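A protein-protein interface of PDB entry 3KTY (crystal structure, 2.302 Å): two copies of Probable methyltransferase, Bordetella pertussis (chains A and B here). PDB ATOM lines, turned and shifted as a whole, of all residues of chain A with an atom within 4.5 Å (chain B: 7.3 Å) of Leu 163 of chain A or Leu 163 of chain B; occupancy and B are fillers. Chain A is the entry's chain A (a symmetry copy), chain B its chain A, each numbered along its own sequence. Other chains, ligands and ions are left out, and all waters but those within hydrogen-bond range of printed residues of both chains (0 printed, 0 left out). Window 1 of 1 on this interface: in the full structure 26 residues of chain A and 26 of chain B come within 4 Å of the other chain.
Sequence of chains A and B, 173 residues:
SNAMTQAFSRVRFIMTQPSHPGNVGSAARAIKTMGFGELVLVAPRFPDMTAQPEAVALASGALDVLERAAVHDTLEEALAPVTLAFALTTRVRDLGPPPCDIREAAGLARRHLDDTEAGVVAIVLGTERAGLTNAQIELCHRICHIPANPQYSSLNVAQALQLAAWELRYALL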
ATOM      1  N   MET A  34      16.999 -31.048  14.960  1.00  0.00           N
ATOM      2  CA  MET A  34      15.903 -31.737  14.302  1.00  0.00           C
ATOM      3  C   MET A  34      16.392 -32.858  13.392  1.00  0.00           C
ATOM      4  O   MET A  34      15.610 -33.512  12.729  1.00  0.00           O
ATOM      5  CB  MET A  34      15.035 -30.727  13.509  1.00  0.00           C
ATOM      6  CG  MET A  34      14.309 -29.669  14.441  1.00  0.00           C
ATOM      7  SD  MET A  34      13.293 -30.563  15.915  1.00  0.00           S
ATOM      8  CE  MET A  34      13.605 -29.254  17.332  1.00  0.00           C
ATOM      9  N   ILE A 146       3.642 -19.804   8.575  1.00  0.00           N
ATOM     10  CA  ILE A 146       3.541 -20.242   9.955  1.00  0.00           C
ATOM     11  C   ILE A 146       2.521 -19.301  10.553  1.00  0.00           C
ATOM     12  O   ILE A 146       2.784 -18.099  10.664  1.00  0.00           O
ATOM     13  CB  ILE A 146       4.888 -20.126  10.659  1.00  0.00           C
ATOM     14  CG1 ILE A 146       5.929 -20.984   9.927  1.00  0.00           C
ATOM     15  CG2 ILE A 146       4.779 -20.531  12.102  1.00  0.00           C
ATOM     16  CD1 ILE A 146       7.143 -21.316  10.747  1.00  0.00           C
ATOM     17  N   GLN A 159      13.887 -19.062  14.624  1.00  0.00           N
ATOM     18  CA  GLN A 159      12.717 -19.638  15.271  1.00  0.00           C
ATOM     19  C   GLN A 159      11.763 -20.178  14.215  1.00  0.00           C
ATOM     20  O   GLN A 159      11.358 -21.342  14.280  1.00  0.00           O
ATOM     21  CB  GLN A 159      12.075 -18.602  16.165  1.00  0.00           C
ATOM     22  CG  GLN A 159      12.998 -18.247  17.341  1.00  0.00           C
ATOM     23  CD  GLN A 159      12.717 -16.875  17.953  1.00  0.00           C
ATOM     24  OE1 GLN A 159      11.652 -16.276  17.721  1.00  0.00           O
ATOM     25  NE2 GLN A 159      13.675 -16.372  18.748  1.00  0.00           N
ATOM     26  N   ALA A 160      11.479 -19.365  13.197  1.00  0.00           N
ATOM     27  CA  ALA A 160      10.802 -19.867  12.023  1.00  0.00           C
ATOM     28  C   ALA A 160      11.447 -21.182  11.579  1.00  0.00           C
ATOM     29  O   ALA A 160      10.756 -22.181  11.383  1.00  0.00           O
ATOM     30  CB  ALA A 160      10.811 -18.876  10.902  1.00  0.00           C
ATOM     31  N   LEU A 161      12.771 -21.191  11.480  1.00  0.00           N
ATOM     32  CA  LEU A 161      13.487 -22.390  11.044  1.00  0.00           C
ATOM     33  C   LEU A 161      13.277 -23.585  11.969  1.00  0.00           C
ATOM     34  O   LEU A 161      13.089 -24.726  11.512  1.00  0.00           O
ATOM     35  CB  LEU A 161      14.983 -22.127  10.909  1.00  0.00           C
ATOM     36  CG  LEU A 161      15.374 -21.813   9.490  1.00  0.00           C
ATOM     37  CD1 LEU A 161      16.880 -21.807   9.353  1.00  0.00           C
ATOM     38  CD2 LEU A 161      14.774 -22.841   8.600  1.00  0.00           C
ATOM     39  N   GLN A 162      13.351 -23.352  13.267  1.00  0.00           N
ATOM     40  CA  GLN A 162      13.161 -24.465  14.172  1.00  0.00           C
ATOM     41  C   GLN A 162      11.737 -25.077  14.005  1.00  0.00           C
ATOM     42  O   GLN A 162      11.575 -26.309  13.927  1.00  0.00           O
ATOM     43  CB  GLN A 162      13.425 -24.024  15.610  1.00  0.00           C
ATOM     44  CG  GLN A 162      13.733 -25.178  16.536  1.00  0.00           C
ATOM     45  CD  GLN A 162      13.951 -24.716  17.962  1.00  0.00           C
ATOM     46  OE1 GLN A 162      14.307 -25.510  18.844  1.00  0.00           O
ATOM     47  NE2 GLN A 162      13.742 -23.417  18.200  1.00  0.00           N
ATOM     48  N   LEU A 163      10.717 -24.215  13.943  1.00  0.00           N
ATOM     49  CA  LEU A 163       9.375 -24.708  13.719  1.00  0.00           C
ATOM     50  C   LEU A 163       9.330 -25.544  12.427  1.00  0.00           C
ATOM     51  O   LEU A 163       8.833 -26.646  12.438  1.00  0.00           O
ATOM     52  CB  LEU A 163       8.330 -23.578  13.713  1.00  0.00           C
ATOM     53  CG  LEU A 163       8.163 -22.970  15.075  1.00  0.00           C
ATOM     54  CD1 LEU A 163       6.979 -22.060  15.096  1.00  0.00           C
ATOM     55  CD2 LEU A 163       8.014 -24.067  16.091  1.00  0.00           C
ATOM     56  N   ALA A 164       9.827 -25.008  11.323  1.00  0.00           N
ATOM     57  CA  ALA A 164       9.803 -25.740  10.047  1.00  0.00           C
ATOM     58  C   ALA A 164      10.503 -27.091  10.124  1.00  0.00           C
ATOM     59  O   ALA A 164      10.008 -28.126   9.660  1.00  0.00           O
ATOM     60  CB  ALA A 164      10.453 -24.914   8.979  1.00  0.00           C
ATOM     61  N   ALA A 165      11.673 -27.073  10.740  1.00  0.00           N
ATOM     62  CA  ALA A 165      12.451 -28.264  10.867  1.00  0.00           C
ATOM     63  C   ALA A 165      11.781 -29.253  11.824  1.00  0.00           C
ATOM     64  O   ALA A 165      11.899 -30.458  11.641  1.00  0.00           O
ATOM     65  CB  ALA A 165      13.885 -27.925  11.326  1.00  0.00           C
ATOM     66  N   TRP A 166      11.090 -28.752  12.849  1.00  0.00           N
ATOM     67  CA  TRP A 166      10.342 -29.657  13.728  1.00  0.00           C
ATOM     68  C   TRP A 166       9.197 -30.332  12.926  1.00  0.00           C
ATOM     69  O   TRP A 166       9.075 -31.552  12.897  1.00  0.00           O
ATOM     70  CB  TRP A 166       9.883 -28.926  15.042  1.00  0.00           C
ATOM     71  CG  TRP A 166       8.705 -29.525  15.584  1.00  0.00           C
ATOM     72  CD1 TRP A 166       7.456 -29.030  15.528  1.00  0.00           C
ATOM     73  CD2 TRP A 166       8.609 -30.815  16.198  1.00  0.00           C
ATOM     74  NE1 TRP A 166       6.568 -29.916  16.089  1.00  0.00           N
ATOM     75  CE2 TRP A 166       7.252 -31.027  16.509  1.00  0.00           C
ATOM     76  CE3 TRP A 166       9.544 -31.819  16.509  1.00  0.00           C
ATOM     77  CZ2 TRP A 166       6.786 -32.198  17.100  1.00  0.00           C
ATOM     78  CZ3 TRP A 166       9.086 -32.986  17.114  1.00  0.00           C
ATOM     79  CH2 TRP A 166       7.723 -33.158  17.405  1.00  0.00           C
ATOM     80  N   GLU A 167       8.397 -29.549  12.223  1.00  0.00           N
ATOM     81  CA  GLU A 167       7.328 -30.107  11.357  1.00  0.00           C
ATOM     82  C   GLU A 167       7.814 -31.150  10.361  1.00  0.00           C
ATOM     83  O   GLU A 167       7.220 -32.228  10.189  1.00  0.00           O
ATOM     84  CB  GLU A 167       6.670 -28.963  10.600  1.00  0.00           C
ATOM     85  CG  GLU A 167       5.733 -28.122  11.576  1.00  0.00           C
ATOM     86  CD  GLU A 167       4.493 -28.887  12.071  1.00  0.00           C
ATOM     87  OE1 GLU A 167       4.123 -29.916  11.475  1.00  0.00           O
ATOM     88  OE2 GLU A 167       3.869 -28.465  13.067  1.00  0.00           O
ATOM     89  N   PHE B  13       2.254 -22.420  31.198  1.00  0.00           N
ATOM     90  CA  PHE B  13       3.588 -23.029  31.056  1.00  0.00           C
ATOM     91  C   PHE B  13       4.405 -22.840  32.316  1.00  0.00           C
ATOM     92  O   PHE B  13       4.689 -21.724  32.741  1.00  0.00           O
ATOM     93  CB  PHE B  13       4.341 -22.445  29.850  1.00  0.00           C
ATOM     94  CG  PHE B  13       3.587 -22.581  28.550  1.00  0.00           C
ATOM     95  CD1 PHE B  13       3.898 -23.584  27.656  1.00  0.00           C
ATOM     96  CD2 PHE B  13       2.534 -21.741  28.262  1.00  0.00           C
ATOM     97  CE1 PHE B  13       3.189 -23.731  26.470  1.00  0.00           C
ATOM     98  CE2 PHE B  13       1.833 -21.866  27.090  1.00  0.00           C
ATOM     99  CZ  PHE B  13       2.152 -22.860  26.198  1.00  0.00           C
ATOM    100  N   ALA B  30       8.961 -16.432  23.664  1.00  0.00           N
ATOM    101  CA  ALA B  30       8.478 -17.670  23.032  1.00  0.00           C
ATOM    102  C   ALA B  30       6.955 -17.863  23.173  1.00  0.00           C
ATOM    103  O   ALA B  30       6.261 -18.000  22.174  1.00  0.00           O
ATOM    104  CB  ALA B  30       9.207 -18.877  23.602  1.00  0.00           C
ATOM    105  N   THR B  33       4.692 -15.263  21.363  1.00  0.00           N
ATOM    106  CA  THR B  33       4.634 -15.369  19.907  1.00  0.00           C
ATOM    107  C   THR B  33       3.622 -16.403  19.432  1.00  0.00           C
ATOM    108  O   THR B  33       3.171 -16.351  18.292  1.00  0.00           O
ATOM    109  CB  THR B  33       6.008 -15.682  19.227  1.00  0.00           C
ATOM    110  OG1 THR B  33       6.413 -17.033  19.508  1.00  0.00           O
ATOM    111  CG2 THR B  33       7.050 -14.735  19.696  1.00  0.00           C
ATOM    112  N   MET B  34       3.322 -17.365  20.290  1.00  0.00           N
ATOM    113  CA  MET B  34       2.335 -18.396  20.025  1.00  0.00           C
ATOM    114  C   MET B  34       0.951 -18.015  20.537  1.00  0.00           C
ATOM    115  O   MET B  34       0.014 -18.783  20.437  1.00  0.00           O
ATOM    116  CB  MET B  34       2.794 -19.745  20.636  1.00  0.00           C
ATOM    117  CG  MET B  34       4.118 -20.308  19.969  1.00  0.00           C
ATOM    118  SD  MET B  34       3.963 -20.383  17.976  1.00  0.00           S
ATOM    119  CE  MET B  34       5.802 -19.913  17.513  1.00  0.00           C
ATOM    120  N   LEU B  88       6.655 -32.349  30.517  1.00  0.00           N
ATOM    121  CA  LEU B  88       7.480 -32.359  29.306  1.00  0.00           C
ATOM    122  C   LEU B  88       8.929 -32.847  29.522  1.00  0.00           C
ATOM    123  O   LEU B  88       9.691 -32.296  30.324  1.00  0.00           O
ATOM    124  CB  LEU B  88       7.493 -30.959  28.698  1.00  0.00           C
ATOM    125  CG  LEU B  88       7.914 -30.914  27.232  1.00  0.00           C
ATOM    126  CD1 LEU B  88       7.513 -32.200  26.559  1.00  0.00           C
ATOM    127  CD2 LEU B  88       7.281 -29.742  26.539  1.00  0.00           C
ATOM    128  N   ILE B 102       4.353 -34.768  21.992  1.00  0.00           N
ATOM    129  CA  ILE B 102       3.808 -33.428  22.140  1.00  0.00           C
ATOM    130  C   ILE B 102       2.634 -33.187  21.200  1.00  0.00           C
ATOM    131  O   ILE B 102       1.793 -32.353  21.466  1.00  0.00           O
ATOM    132  CB  ILE B 102       4.918 -32.356  21.912  1.00  0.00           C
ATOM    133  CG1 ILE B 102       4.397 -30.971  22.221  1.00  0.00           C
ATOM    134  CG2 ILE B 102       5.477 -32.413  20.460  1.00  0.00           C
ATOM    135  CD1 ILE B 102       4.090 -30.785  23.689  1.00  0.00           C
ATOM    136  N   ILE B 146       9.346 -34.670  23.422  1.00  0.00           N
ATOM    137  CA  ILE B 146       9.606 -34.101  22.113  1.00  0.00           C
ATOM    138  C   ILE B 146      10.651 -35.021  21.526  1.00  0.00           C
ATOM    139  O   ILE B 146      11.776 -35.075  22.031  1.00  0.00           O
ATOM    140  CB  ILE B 146      10.126 -32.673  22.237  1.00  0.00           C
ATOM    141  CG1 ILE B 146       9.092 -31.809  22.972  1.00  0.00           C
ATOM    142  CG2 ILE B 146      10.444 -32.096  20.886  1.00  0.00           C
ATOM    143  CD1 ILE B 146       9.264 -30.332  22.767  1.00  0.00           C
ATOM    144  N   ALA B 148      13.142 -35.439  19.438  1.00  0.00           N
ATOM    145  CA  ALA B 148      14.113 -34.722  18.622  1.00  0.00           C
ATOM    146  C   ALA B 148      15.292 -35.613  18.355  1.00  0.00           C
ATOM    147  O   ALA B 148      15.397 -36.684  18.934  1.00  0.00           O
ATOM    148  CB  ALA B 148      14.566 -33.451  19.294  1.00  0.00           C
ATOM    149  N   LEU B 155      17.962 -29.838  23.908  1.00  0.00           N
ATOM    150  CA  LEU B 155      17.794 -28.497  23.363  1.00  0.00           C
ATOM    151  C   LEU B 155      17.313 -27.523  24.433  1.00  0.00           C
ATOM    152  O   LEU B 155      16.588 -27.904  25.352  1.00  0.00           O
ATOM    153  CB  LEU B 155      16.813 -28.515  22.188  1.00  0.00           C
ATOM    154  CG  LEU B 155      15.696 -29.558  22.254  1.00  0.00           C
ATOM    155  CD1 LEU B 155      15.284 -29.815  23.696  1.00  0.00           C
ATOM    156  CD2 LEU B 155      14.502 -29.121  21.421  1.00  0.00           C
ATOM    157  N   VAL B 157      15.632 -25.098  26.986  1.00  0.00           N
ATOM    158  CA  VAL B 157      14.299 -25.197  27.538  1.00  0.00           C
ATOM    159  C   VAL B 157      13.394 -24.199  26.840  1.00  0.00           C
ATOM    160  O   VAL B 157      12.211 -24.433  26.663  1.00  0.00           O
ATOM    161  CB  VAL B 157      14.336 -24.935  29.071  1.00  0.00           C
ATOM    162  CG1 VAL B 157      12.946 -24.987  29.701  1.00  0.00           C
ATOM    163  CG2 VAL B 157      15.261 -25.935  29.743  1.00  0.00           C
ATOM    164  N   ALA B 158      13.932 -23.076  26.404  1.00  0.00           N
ATOM    165  CA  ALA B 158      13.051 -22.127  25.736  1.00  0.00           C
ATOM    166  C   ALA B 158      12.654 -22.656  24.340  1.00  0.00           C
ATOM    167  O   ALA B 158      11.611 -22.298  23.802  1.00  0.00           O
ATOM    168  CB  ALA B 158      13.695 -20.751  25.651  1.00  0.00           C
ATOM    169  N   GLN B 159      13.505 -23.504  23.764  1.00  0.00           N
ATOM    170  CA  GLN B 159      13.229 -24.124  22.475  1.00  0.00           C
ATOM    171  C   GLN B 159      12.195 -25.227  22.648  1.00  0.00           C
ATOM    172  O   GLN B 159      11.176 -25.240  21.953  1.00  0.00           O
ATOM    173  CB  GLN B 159      14.522 -24.622  21.869  1.00  0.00           C
ATOM    174  CG  GLN B 159      15.447 -23.448  21.513  1.00  0.00           C
ATOM    175  CD  GLN B 159      16.924 -23.831  21.432  1.00  0.00           C
ATOM    176  OE1 GLN B 159      17.274 -25.022  21.346  1.00  0.00           O
ATOM    177  NE2 GLN B 159      17.803 -22.816  21.452  1.00  0.00           N
ATOM    178  N   ALA B 160      12.412 -26.095  23.637  1.00  0.00           N
ATOM    179  CA  ALA B 160      11.373 -27.011  24.050  1.00  0.00           C
ATOM    180  C   ALA B 160      10.049 -26.259  24.192  1.00  0.00           C
ATOM    181  O   ALA B 160       9.034 -26.670  23.631  1.00  0.00           O
ATOM    182  CB  ALA B 160      11.717 -27.711  25.327  1.00  0.00           C
ATOM    183  N   LEU B 161      10.078 -25.130  24.891  1.00  0.00           N
ATOM    184  CA  LEU B 161       8.864 -24.344  25.106  1.00  0.00           C
ATOM    185  C   LEU B 161       8.236 -23.841  23.810  1.00  0.00           C
ATOM    186  O   LEU B 161       7.005 -23.873  23.638  1.00  0.00           O
ATOM    187  CB  LEU B 161       9.127 -23.152  26.022  1.00  0.00           C
ATOM    188  CG  LEU B 161       8.758 -23.448  27.451  1.00  0.00           C
ATOM    189  CD1 LEU B 161       8.795 -22.179  28.272  1.00  0.00           C
ATOM    190  CD2 LEU B 161       7.396 -24.042  27.471  1.00  0.00           C
ATOM    191  N   GLN B 162       9.058 -23.334  22.910  1.00  0.00           N
ATOM    192  CA  GLN B 162       8.494 -22.844  21.670  1.00  0.00           C
ATOM    193  C   GLN B 162       7.787 -23.994  20.892  1.00  0.00           C
ATOM    194  O   GLN B 162       6.656 -23.830  20.397  1.00  0.00           O
ATOM    195  CB  GLN B 162       9.577 -22.171  20.830  1.00  0.00           C
ATOM    196  CG  GLN B 162       9.019 -21.224  19.793  1.00  0.00           C
ATOM    197  CD  GLN B 162      10.112 -20.602  18.948  1.00  0.00           C
ATOM    198  OE1 GLN B 162       9.853 -19.728  18.109  1.00  0.00           O
ATOM    199  NE2 GLN B 162      11.353 -21.048  19.169  1.00  0.00           N
ATOM    200  N   LEU B 163       8.451 -25.150  20.796  1.00  0.00           N
ATOM    201  CA  LEU B 163       7.826 -26.283  20.147  1.00  0.00           C
ATOM    202  C   LEU B 163       6.478 -26.599  20.822  1.00  0.00           C
ATOM    203  O   LEU B 163       5.483 -26.731  20.148  1.00  0.00           O
ATOM    204  CB  LEU B 163       8.749 -27.513  20.100  1.00  0.00           C
ATOM    205  CG  LEU B 163       9.917 -27.294  19.181  1.00  0.00           C
ATOM    206  CD1 LEU B 163      10.651 -28.576  18.961  1.00  0.00           C
ATOM    207  CD2 LEU B 163       9.422 -26.730  17.879  1.00  0.00           C
ATOM    208  N   ALA B 164       6.460 -26.738  22.138  1.00  0.00           N
ATOM    209  CA  ALA B 164       5.213 -27.058  22.849  1.00  0.00           C
ATOM    210  C   ALA B 164       4.106 -26.043  22.592  1.00  0.00           C
ATOM    211  O   ALA B 164       2.945 -26.377  22.322  1.00  0.00           O
ATOM    212  CB  ALA B 164       5.477 -27.128  24.324  1.00  0.00           C
ATOM    213  N   ALA B 165       4.487 -24.779  22.665  1.00  0.00           N
ATOM    214  CA  ALA B 165       3.549 -23.720  22.467  1.00  0.00           C
ATOM    215  C   ALA B 165       3.088 -23.666  21.008  1.00  0.00           C
ATOM    216  O   ALA B 165       1.949 -23.304  20.738  1.00  0.00           O
ATOM    217  CB  ALA B 165       4.154 -22.373  22.912  1.00  0.00           C
ATOM    218  N   TRP B 166       3.969 -24.010  20.067  1.00  0.00           N
ATOM    219  CA  TRP B 166       3.540 -24.078  18.666  1.00  0.00           C
ATOM    220  C   TRP B 166       2.495 -25.214  18.497  1.00  0.00           C
ATOM    221  O   TRP B 166       1.400 -25.000  17.985  1.00  0.00           O
ATOM    222  CB  TRP B 166       4.773 -24.169  17.695  1.00  0.00           C
ATOM    223  CG  TRP B 166       4.427 -24.830  16.478  1.00  0.00           C
ATOM    224  CD1 TRP B 166       4.757 -26.086  16.125  1.00  0.00           C
ATOM    225  CD2 TRP B 166       3.577 -24.323  15.443  1.00  0.00           C
ATOM    226  NE1 TRP B 166       4.185 -26.405  14.918  1.00  0.00           N
ATOM    227  CE2 TRP B 166       3.451 -25.337  14.475  1.00  0.00           C
ATOM    228  CE3 TRP B 166       2.900 -23.105  15.247  1.00  0.00           C
ATOM    229  CZ2 TRP B 166       2.669 -25.196  13.330  1.00  0.00           C
ATOM    230  CZ3 TRP B 166       2.130 -22.953  14.097  1.00  0.00           C
ATOM    231  CH2 TRP B 166       2.030 -23.991  13.157  1.00  0.00           C
ATOM    232  N   GLU B 167       2.800 -26.405  18.980  1.00  0.00           N
ATOM    233  CA  GLU B 167       1.833 -27.531  18.943  1.00  0.00           C
ATOM    234  C   GLU B 167       0.477 -27.207  19.553  1.00  0.00           C
ATOM    235  O   GLU B 167      -0.590 -27.502  18.988  1.00  0.00           O
ATOM    236  CB  GLU B 167       2.440 -28.717  19.677  1.00  0.00           C
ATOM    237  CG  GLU B 167       3.581 -29.390  18.792  1.00  0.00           C
ATOM    238  CD  GLU B 167       3.062 -30.078  17.516  1.00  0.00           C
ATOM    239  OE1 GLU B 167       1.852 -30.356  17.412  1.00  0.00           O
ATOM    240  OE2 GLU B 167       3.864 -30.354  16.600  1.00  0.00           O
ATOM    241  N   LEU B 168       0.529 -26.558  20.710  1.00  0.00           N
ATOM    242  CA  LEU B 168      -0.666 -26.156  21.396  1.00  0.00           C
ATOM    243  C   LEU B 168      -1.420 -25.113  20.624  1.00  0.00           C
ATOM    244  O   LEU B 168      -2.620 -25.174  20.486  1.00  0.00           O
ATOM    245  CB  LEU B 168      -0.326 -25.636  22.788  1.00  0.00           C
ATOM    246  CG  LEU B 168      -0.064 -26.775  23.775  1.00  0.00           C
ATOM    247  CD1 LEU B 168       0.476 -26.198  25.050  1.00  0.00           C
ATOM    248  CD2 LEU B 168      -1.369 -27.515  24.010  1.00  0.00           C
ATOM    249  N   ARG B 169      -0.719 -24.132  20.116  1.00  0.00           N
ATOM    250  CA  ARG B 169      -1.400 -23.151  19.299  1.00  0.00           C
ATOM    251  C   ARG B 169      -2.108 -23.812  18.111  1.00  0.00           C
ATOM    252  O   ARG B 169      -3.282 -23.567  17.818  1.00  0.00           O
ATOM    253  CB  ARG B 169      -0.384 -22.109  18.808  1.00  0.00           C
ATOM    254  CG  ARG B 169      -0.921 -21.189  17.750  1.00  0.00           C
ATOM    255  CD  ARG B 169       0.088 -20.003  17.463  1.00  0.00           C
ATOM    256  NE  ARG B 169      -0.596 -19.073  16.584  1.00  0.00           N
ATOM    257  CZ  ARG B 169      -1.507 -18.198  16.982  1.00  0.00           C
ATOM    258  NH1 ARG B 169      -1.802 -18.077  18.261  1.00  0.00           N
ATOM    259  NH2 ARG B 169      -2.125 -17.442  16.097  1.00  0.00           N
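OE2 of Glu 167 of chain B sits at hydrogen-bond distance from NE1 of Trp 166 of chain A (2.8 Å).
The indole nitrogen (NE1) of Trp 166 of chain B lies within hydrogen-bond range of the side-chain carboxylate (OE2) of Glu 167 of chain A, 2.8 Å away.
The guanidinium group (NH1) of Arg 169 of chain B is in hydrogen-bond range of the backbone carbonyl oxygen (O) of Met 34 of chain B (2.9 Å).
Among the printed residues, merely in contact across the chains: Gln 159 of chain A with Gln 162 of chain B, Gln 162 of chain A with Gln 159 of chain B, Leu 163 of chain A with Met 34 of chain B, Met 34 of chain A with Leu 163 of chain B, Gln 162 of chain A with Gln 162 of chain B, Leu 163 of chain A with Leu 163 of chain B, Trp 166 of chain A with Ile 102 of chain B, Trp 166 of chain A with Leu 163 of chain B and Leu 163 of chain A with Trp 166 of chain B.
Of the printed residues of chain B, Met 34 of chain A touches Leu 163.
Of the printed residues of chain B, Leu 163 of chain A touches Met 34, Leu 163 and Trp 166.
Printed residues of chain A within 4 Å of Gln 162 of chain B: Gln 159 and Gln 162.
Of the printed residues of chain A, Leu 163 of chain B touches Met 34, Leu 163 and Trp 166.
Printed residues of chain A within 4 Å of Glu 167 of chain B: Trp 166 (2.8 Å).
The nearest residue of chain B that does not touch Leu 163 of chain A is Gln 162 of chain B (4.5 Å).
The nearest printed residue of chain B that does not touch Glu 167 of chain A is Glu 167 of chain B (4.01 Å).
Met 34 of chain A touches Leu 163 of chain B, and with the chains exchanged Leu 163 of chain A touches Met 34 of chain B.
Gln 159 of chain A touches Gln 162 of chain B, and with the chains exchanged Gln 162 of chain A touches Gln 159 of chain B.
Gln 162 of chain A touches its own counterpart, Gln 162 of chain B.
Leu 163 of chain B touches its own counterpart, Leu 163 of chain A.
Of the 11 pairs that touch across the chains among the printed residues, 10 have their exchanged pair printed and touching as well.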
